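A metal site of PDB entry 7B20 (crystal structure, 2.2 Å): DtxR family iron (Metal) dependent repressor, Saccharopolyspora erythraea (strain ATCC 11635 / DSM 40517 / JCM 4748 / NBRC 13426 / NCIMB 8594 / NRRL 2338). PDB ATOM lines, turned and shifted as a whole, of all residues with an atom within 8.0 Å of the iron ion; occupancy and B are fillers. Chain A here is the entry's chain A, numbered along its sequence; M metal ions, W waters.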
ATOM      1  N   ASP A   5       4.971  -3.445   7.592  1.00  0.00           N
ATOM      2  CA  ASP A   5       4.289  -4.509   6.803  1.00  0.00           C
ATOM      3  C   ASP A   5       4.728  -5.883   7.349  1.00  0.00           C
ATOM      4  O   ASP A   5       3.857  -6.605   7.863  1.00  0.00           O
ATOM      5  CB  ASP A   5       4.592  -4.364   5.301  1.00  0.00           C
ATOM      6  CG  ASP A   5       3.628  -5.085   4.386  1.00  0.00           C
ATOM      7  OD1 ASP A   5       2.970  -6.047   4.851  1.00  0.00           O
ATOM      8  OD2 ASP A   5       3.538  -4.693   3.206  1.00  0.00           O
ATOM      9  N   LEU A   6       6.024  -6.190   7.263  1.00  0.00           N
ATOM     10  CA  LEU A   6       6.627  -7.479   7.726  1.00  0.00           C
ATOM     11  C   LEU A   6       6.974  -7.402   9.212  1.00  0.00           C
ATOM     12  O   LEU A   6       7.197  -8.464   9.817  1.00  0.00           O
ATOM     13  CB  LEU A   6       7.889  -7.771   6.898  1.00  0.00           C
ATOM     14  CG  LEU A   6       7.672  -7.974   5.393  1.00  0.00           C
ATOM     15  CD1 LEU A   6       9.008  -8.183   4.694  1.00  0.00           C
ATOM     16  CD2 LEU A   6       6.745  -9.155   5.128  1.00  0.00           C
ATOM     17  N   ILE A   7       7.034  -6.181   9.771  1.00  0.00           N
ATOM     18  CA  ILE A   7       7.400  -5.885  11.195  1.00  0.00           C
ATOM     19  C   ILE A   7       8.911  -6.077  11.377  1.00  0.00           C
ATOM     20  O   ILE A   7       9.570  -5.109  11.825  1.00  0.00           O
ATOM     21  CB  ILE A   7       6.583  -6.735  12.191  1.00  0.00           C
ATOM     22  CG1 ILE A   7       5.076  -6.622  11.957  1.00  0.00           C
ATOM     23  CG2 ILE A   7       6.962  -6.374  13.622  1.00  0.00           C
ATOM     24  CD1 ILE A   7       4.525  -5.220  12.079  1.00  0.00           C
ATOM     25  N   ASP A   8       9.439  -7.260  11.050  1.00  0.00           N
ATOM     26  CA  ASP A   8      10.882  -7.614  11.132  1.00  0.00           C
ATOM     27  C   ASP A   8      11.285  -8.365   9.858  1.00  0.00           C
ATOM     28  O   ASP A   8      10.915  -9.553   9.724  1.00  0.00           O
ATOM     29  CB  ASP A   8      11.182  -8.415  12.396  1.00  0.00           C
ATOM     30  CG  ASP A   8      12.670  -8.546  12.729  1.00  0.00           C
ATOM     31  OD1 ASP A   8      13.473  -8.733  11.789  1.00  0.00           O
ATOM     32  OD2 ASP A   8      13.004  -8.468  13.927  1.00  0.00           O
ATOM     33  N   GLU A  11      13.635 -11.646  10.422  1.00  0.00           N
ATOM     34  CA  GLU A  11      12.891 -12.782  11.043  1.00  0.00           C
ATOM     35  C   GLU A  11      11.971 -13.423   9.997  1.00  0.00           C
ATOM     36  O   GLU A  11      11.813 -14.656  10.034  1.00  0.00           O
ATOM     37  CB  GLU A  11      12.098 -12.311  12.268  1.00  0.00           C
ATOM     38  CG  GLU A  11      12.981 -12.025  13.469  1.00  0.00           C
ATOM     39  CD  GLU A  11      12.248 -11.736  14.778  1.00  0.00           C
ATOM     40  OE1 GLU A  11      11.019 -11.531  14.743  1.00  0.00           O
ATOM     41  OE2 GLU A  11      12.917 -11.732  15.823  1.00  0.00           O
ATOM     42  N   MET A  12      11.389 -12.617   9.100  1.00  0.00           N
ATOM     43  CA  MET A  12      10.415 -13.111   8.086  1.00  0.00           C
ATOM     44  C   MET A  12      11.165 -13.840   6.960  1.00  0.00           C
ATOM     45  O   MET A  12      10.587 -14.816   6.435  1.00  0.00           O
ATOM     46  CB  MET A  12       9.573 -11.970   7.504  1.00  0.00           C
ATOM     47  CG  MET A  12       8.337 -11.665   8.338  1.00  0.00           C
ATOM     48  SD  MET A  12       7.283 -13.122   8.640  1.00  0.00           S
ATOM     49  CE  MET A  12       6.595 -13.382   7.003  1.00  0.00           C
ATOM     50  N   TYR A  13      12.383 -13.412   6.628  1.00  0.00           N
ATOM     51  CA  TYR A  13      13.272 -14.122   5.667  1.00  0.00           C
ATOM     52  C   TYR A  13      13.676 -15.474   6.259  1.00  0.00           C
ATOM     53  O   TYR A  13      13.624 -16.492   5.537  1.00  0.00           O
ATOM     54  CB  TYR A  13      14.499 -13.278   5.307  1.00  0.00           C
ATOM     55  CG  TYR A  13      14.297 -12.336   4.152  1.00  0.00           C
ATOM     56  CD1 TYR A  13      13.247 -11.425   4.145  1.00  0.00           C
ATOM     57  CD2 TYR A  13      15.160 -12.326   3.072  1.00  0.00           C
ATOM     58  CE1 TYR A  13      13.058 -10.545   3.094  1.00  0.00           C
ATOM     59  CE2 TYR A  13      14.989 -11.457   2.010  1.00  0.00           C
ATOM     60  CZ  TYR A  13      13.933 -10.565   2.018  1.00  0.00           C
ATOM     61  OH  TYR A  13      13.742  -9.691   0.980  1.00  0.00           O
ATOM     62  N   ARG A  15      12.086 -17.232   8.694  1.00  0.00           N
ATOM     63  CA  ARG A  15      10.901 -18.115   8.837  1.00  0.00           C
ATOM     64  C   ARG A  15      10.465 -18.594   7.442  1.00  0.00           C
ATOM     65  O   ARG A  15      10.051 -19.764   7.353  1.00  0.00           O
ATOM     66  CB  ARG A  15       9.750 -17.416   9.568  1.00  0.00           C
ATOM     67  CG  ARG A  15       8.874 -18.384  10.351  1.00  0.00           C
ATOM     68  CD  ARG A  15       7.431 -17.925  10.473  1.00  0.00           C
ATOM     69  NE  ARG A  15       6.688 -18.123   9.234  1.00  0.00           N
ATOM     70  CZ  ARG A  15       5.619 -17.424   8.858  1.00  0.00           C
ATOM     71  NH1 ARG A  15       5.119 -16.464   9.629  1.00  0.00           N
ATOM     72  NH2 ARG A  15       5.035 -17.694   7.696  1.00  0.00           N
ATOM     73  N   THR A  16      10.555 -17.748   6.416  1.00  0.00           N
ATOM     74  CA  THR A  16      10.195 -18.091   5.010  1.00  0.00           C
ATOM     75  C   THR A  16      11.105 -19.220   4.520  1.00  0.00           C
ATOM     76  O   THR A  16      10.592 -20.141   3.869  1.00  0.00           O
ATOM     77  CB  THR A  16      10.271 -16.889   4.067  1.00  0.00           C
ATOM     78  OG1 THR A  16       9.282 -15.937   4.479  1.00  0.00           O
ATOM     79  CG2 THR A  16      10.022 -17.257   2.625  1.00  0.00           C
ATOM     80  N   LEU A  36       6.881 -13.209  -0.143  1.00  0.00           N
ATOM     81  CA  LEU A  36       6.841 -11.913   0.576  1.00  0.00           C
ATOM     82  C   LEU A  36       6.499 -10.772  -0.396  1.00  0.00           C
ATOM     83  O   LEU A  36       6.397  -9.619   0.082  1.00  0.00           O
ATOM     84  CB  LEU A  36       8.189 -11.674   1.263  1.00  0.00           C
ATOM     85  CG  LEU A  36       8.627 -12.746   2.265  1.00  0.00           C
ATOM     86  CD1 LEU A  36       9.907 -12.347   2.974  1.00  0.00           C
ATOM     87  CD2 LEU A  36       7.532 -13.025   3.278  1.00  0.00           C
ATOM     88  N   VAL A  77      11.433 -17.907  16.165  1.00  0.00           N
ATOM     89  CA  VAL A  77      10.319 -17.167  15.509  1.00  0.00           C
ATOM     90  C   VAL A  77       9.159 -18.131  15.235  1.00  0.00           C
ATOM     91  O   VAL A  77       7.997 -17.753  15.500  1.00  0.00           O
ATOM     92  CB  VAL A  77      10.796 -16.464  14.216  1.00  0.00           C
ATOM     93  CG1 VAL A  77       9.633 -15.919  13.398  1.00  0.00           C
ATOM     94  CG2 VAL A  77      11.792 -15.357  14.522  1.00  0.00           C
ATOM     95  N   HIS A  81       5.341 -18.204  16.801  1.00  0.00           N
ATOM     96  CA  HIS A  81       4.245 -18.169  15.802  1.00  0.00           C
ATOM     97  C   HIS A  81       3.186 -19.219  16.141  1.00  0.00           C
ATOM     98  O   HIS A  81       1.991 -18.866  16.152  1.00  0.00           O
ATOM     99  CB  HIS A  81       4.811 -18.378  14.388  1.00  0.00           C
ATOM    100  CG  HIS A  81       3.751 -18.437  13.333  1.00  0.00           C
ATOM    101  ND1 HIS A  81       3.176 -17.296  12.806  1.00  0.00           N
ATOM    102  CD2 HIS A  81       3.159 -19.481  12.723  1.00  0.00           C
ATOM    103  CE1 HIS A  81       2.261 -17.644  11.916  1.00  0.00           C
ATOM    104  NE2 HIS A  81       2.248 -18.982  11.844  1.00  0.00           N
ATOM    105  N   HIS A 100      -3.475 -17.165  11.331  1.00  0.00           N
ATOM    106  CA  HIS A 100      -2.082 -17.181  10.809  1.00  0.00           C
ATOM    107  C   HIS A 100      -1.570 -15.746  10.627  1.00  0.00           C
ATOM    108  O   HIS A 100      -0.450 -15.477  11.097  1.00  0.00           O
ATOM    109  CB  HIS A 100      -1.990 -17.973   9.498  1.00  0.00           C
ATOM    110  CG  HIS A 100      -0.663 -17.812   8.834  1.00  0.00           C
ATOM    111  ND1 HIS A 100       0.471 -18.470   9.279  1.00  0.00           N
ATOM    112  CD2 HIS A 100      -0.278 -17.068   7.771  1.00  0.00           C
ATOM    113  CE1 HIS A 100       1.492 -18.132   8.522  1.00  0.00           C
ATOM    114  NE2 HIS A 100       1.065 -17.275   7.594  1.00  0.00           N
ATOM    115  N   LEU A 101      -2.353 -14.876   9.988  1.00  0.00           N
ATOM    116  CA  LEU A 101      -1.942 -13.483   9.665  1.00  0.00           C
ATOM    117  C   LEU A 101      -1.729 -12.685  10.966  1.00  0.00           C
ATOM    118  O   LEU A 101      -0.842 -11.809  10.974  1.00  0.00           O
ATOM    119  CB  LEU A 101      -3.007 -12.819   8.783  1.00  0.00           C
ATOM    120  CG  LEU A 101      -2.698 -11.386   8.348  1.00  0.00           C
ATOM    121  CD1 LEU A 101      -1.397 -11.315   7.556  1.00  0.00           C
ATOM    122  CD2 LEU A 101      -3.843 -10.792   7.546  1.00  0.00           C
ATOM    123  N   GLU A 102      -2.502 -12.993  12.009  1.00  0.00           N
ATOM    124  CA  GLU A 102      -2.348 -12.388  13.358  1.00  0.00           C
ATOM    125  C   GLU A 102      -1.038 -12.911  13.969  1.00  0.00           C
ATOM    126  O   GLU A 102      -0.205 -12.076  14.375  1.00  0.00           O
ATOM    127  CB  GLU A 102      -3.536 -12.741  14.254  1.00  0.00           C
ATOM    128  CG  GLU A 102      -3.666 -11.834  15.467  1.00  0.00           C
ATOM    129  CD  GLU A 102      -4.196 -10.439  15.183  1.00  0.00           C
ATOM    130  OE1 GLU A 102      -4.906 -10.271  14.166  1.00  0.00           O
ATOM    131  OE2 GLU A 102      -3.913  -9.518  15.975  1.00  0.00           O
ATOM    132  N   ALA A 103      -0.874 -14.230  14.010  1.00  0.00           N
ATOM    133  CA  ALA A 103       0.293 -14.941  14.589  1.00  0.00           C
ATOM    134  C   ALA A 103       1.564 -14.560  13.843  1.00  0.00           C
ATOM    135  O   ALA A 103       2.651 -14.619  14.449  1.00  0.00           O
ATOM    136  CB  ALA A 103       0.052 -16.437  14.541  1.00  0.00           C
ATOM    137  N   CYS A 104       1.464 -14.184  12.561  1.00  0.00           N
ATOM    138  CA  CYS A 104       2.609 -13.783  11.699  1.00  0.00           C
ATOM    139  C   CYS A 104       3.195 -12.461  12.195  1.00  0.00           C
ATOM    140  O   CYS A 104       4.390 -12.227  11.984  1.00  0.00           O
ATOM    141  CB  CYS A 104       2.193 -13.676  10.238  1.00  0.00           C
ATOM    142  SG  CYS A 104       3.603 -13.525   9.115  1.00  0.00           S
ATOM    143  N   ARG A 105       2.374 -11.606  12.822  1.00  0.00           N
ATOM    144  CA  ARG A 105       2.813 -10.301  13.386  1.00  0.00           C
ATOM    145  C   ARG A 105       3.252 -10.506  14.844  1.00  0.00           C
ATOM    146  O   ARG A 105       4.244  -9.864  15.242  1.00  0.00           O
ATOM    147  CB  ARG A 105       1.694  -9.260  13.287  1.00  0.00           C
ATOM    148  CG  ARG A 105       1.366  -8.826  11.869  1.00  0.00           C
ATOM    149  CD  ARG A 105       0.549  -7.548  11.841  1.00  0.00           C
ATOM    150  NE  ARG A 105      -0.645  -7.648  12.665  1.00  0.00           N
ATOM    151  CZ  ARG A 105      -1.756  -8.290  12.331  1.00  0.00           C
ATOM    152  NH1 ARG A 105      -1.855  -8.926  11.172  1.00  0.00           N
ATOM    153  NH2 ARG A 105      -2.785  -8.308  13.163  1.00  0.00           N
ATOM    154  N   TRP A 106       2.542 -11.351  15.600  1.00  0.00           N
ATOM    155  CA  TRP A 106       2.781 -11.605  17.047  1.00  0.00           C
ATOM    156  C   TRP A 106       4.127 -12.297  17.264  1.00  0.00           C
ATOM    157  O   TRP A 106       4.720 -12.103  18.352  1.00  0.00           O
ATOM    158  CB  TRP A 106       1.636 -12.425  17.648  1.00  0.00           C
ATOM    159  CG  TRP A 106       0.377 -11.657  17.906  1.00  0.00           C
ATOM    160  CD1 TRP A 106      -0.138 -10.642  17.161  1.00  0.00           C
ATOM    161  CD2 TRP A 106      -0.556 -11.878  18.978  1.00  0.00           C
ATOM    162  NE1 TRP A 106      -1.322 -10.202  17.702  1.00  0.00           N
ATOM    163  CE2 TRP A 106      -1.600 -10.943  18.819  1.00  0.00           C
ATOM    164  CE3 TRP A 106      -0.602 -12.761  20.068  1.00  0.00           C
ATOM    165  CZ2 TRP A 106      -2.670 -10.874  19.696  1.00  0.00           C
ATOM    166  CZ3 TRP A 106      -1.670 -12.695  20.936  1.00  0.00           C
ATOM    167  CH2 TRP A 106      -2.687 -11.751  20.752  1.00  0.00           C
ATOM    168  N   GLU A 107       4.592 -13.086  16.288  1.00  0.00           N
ATOM    169  CA  GLU A 107       5.833 -13.902  16.389  1.00  0.00           C
ATOM    170  C   GLU A 107       7.061 -13.013  16.625  1.00  0.00           C
ATOM    171  O   GLU A 107       8.063 -13.529  17.151  1.00  0.00           O
ATOM    172  CB  GLU A 107       6.014 -14.768  15.127  1.00  0.00           C
ATOM    173  CG  GLU A 107       6.360 -13.975  13.875  1.00  0.00           C
ATOM    174  CD  GLU A 107       6.195 -14.726  12.567  1.00  0.00           C
ATOM    175  OE1 GLU A 107       5.715 -15.872  12.601  1.00  0.00           O
ATOM    176  OE2 GLU A 107       6.537 -14.165  11.513  1.00  0.00           O
ATOM    177  N   HIS A 108       6.990 -11.731  16.261  1.00  0.00           N
ATOM    178  CA  HIS A 108       8.135 -10.778  16.273  1.00  0.00           C
ATOM    179  C   HIS A 108       8.224 -10.021  17.602  1.00  0.00           C
ATOM    180  O   HIS A 108       9.263  -9.383  17.830  1.00  0.00           O
ATOM    181  CB  HIS A 108       8.035  -9.817  15.086  1.00  0.00           C
ATOM    182  CG  HIS A 108       7.878 -10.509  13.774  1.00  0.00           C
ATOM    183  ND1 HIS A 108       8.866 -11.313  13.235  1.00  0.00           N
ATOM    184  CD2 HIS A 108       6.850 -10.521  12.899  1.00  0.00           C
ATOM    185  CE1 HIS A 108       8.452 -11.786  12.085  1.00  0.00           C
ATOM    186  NE2 HIS A 108       7.217 -11.328  11.854  1.00  0.00           N
HETATM  187 FE    FE M   1       5.736 -12.457  10.483  1.00  0.00          FE
HETATM  188  O   HOH W   1       4.801 -10.061   9.617  1.00  0.00           O
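SG of Cys 104 lies close to NH1 of Arg 15 (3.3 Å). The side-chain carboxylate of Glu 107 lies within salt-bridge range of the guanidinium group of Arg 15, 3.1 Å away. The side-chain carboxylate of Glu 107 lies within hydrogen-bond range of a ring nitrogen (ND1) of His 81 (2.9 Å). The side-chain carboxylate of Glu 11 lies within hydrogen-bond range of a ring nitrogen (ND1) of His 108, 2.6 Å away. O of Met 12 sits at hydrogen-bond distance from OG1 of Thr 16 (2.6 Å).
The nearest printed residue that does not touch the iron ion is Arg 15 (4.1 Å).
The iron ion is bound by O of Cys 104 (2.0 Å), OE2 of Glu 107 (2.1 Å), NE2 of His 108 (2.3 Å), SD of Met 12 (2.5 Å) and SG of Cys 104 (2.7 Å). The iron ion has five donor atoms within binding distance. Slightly farther from the iron ion lies water W1 (2.7 Å).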
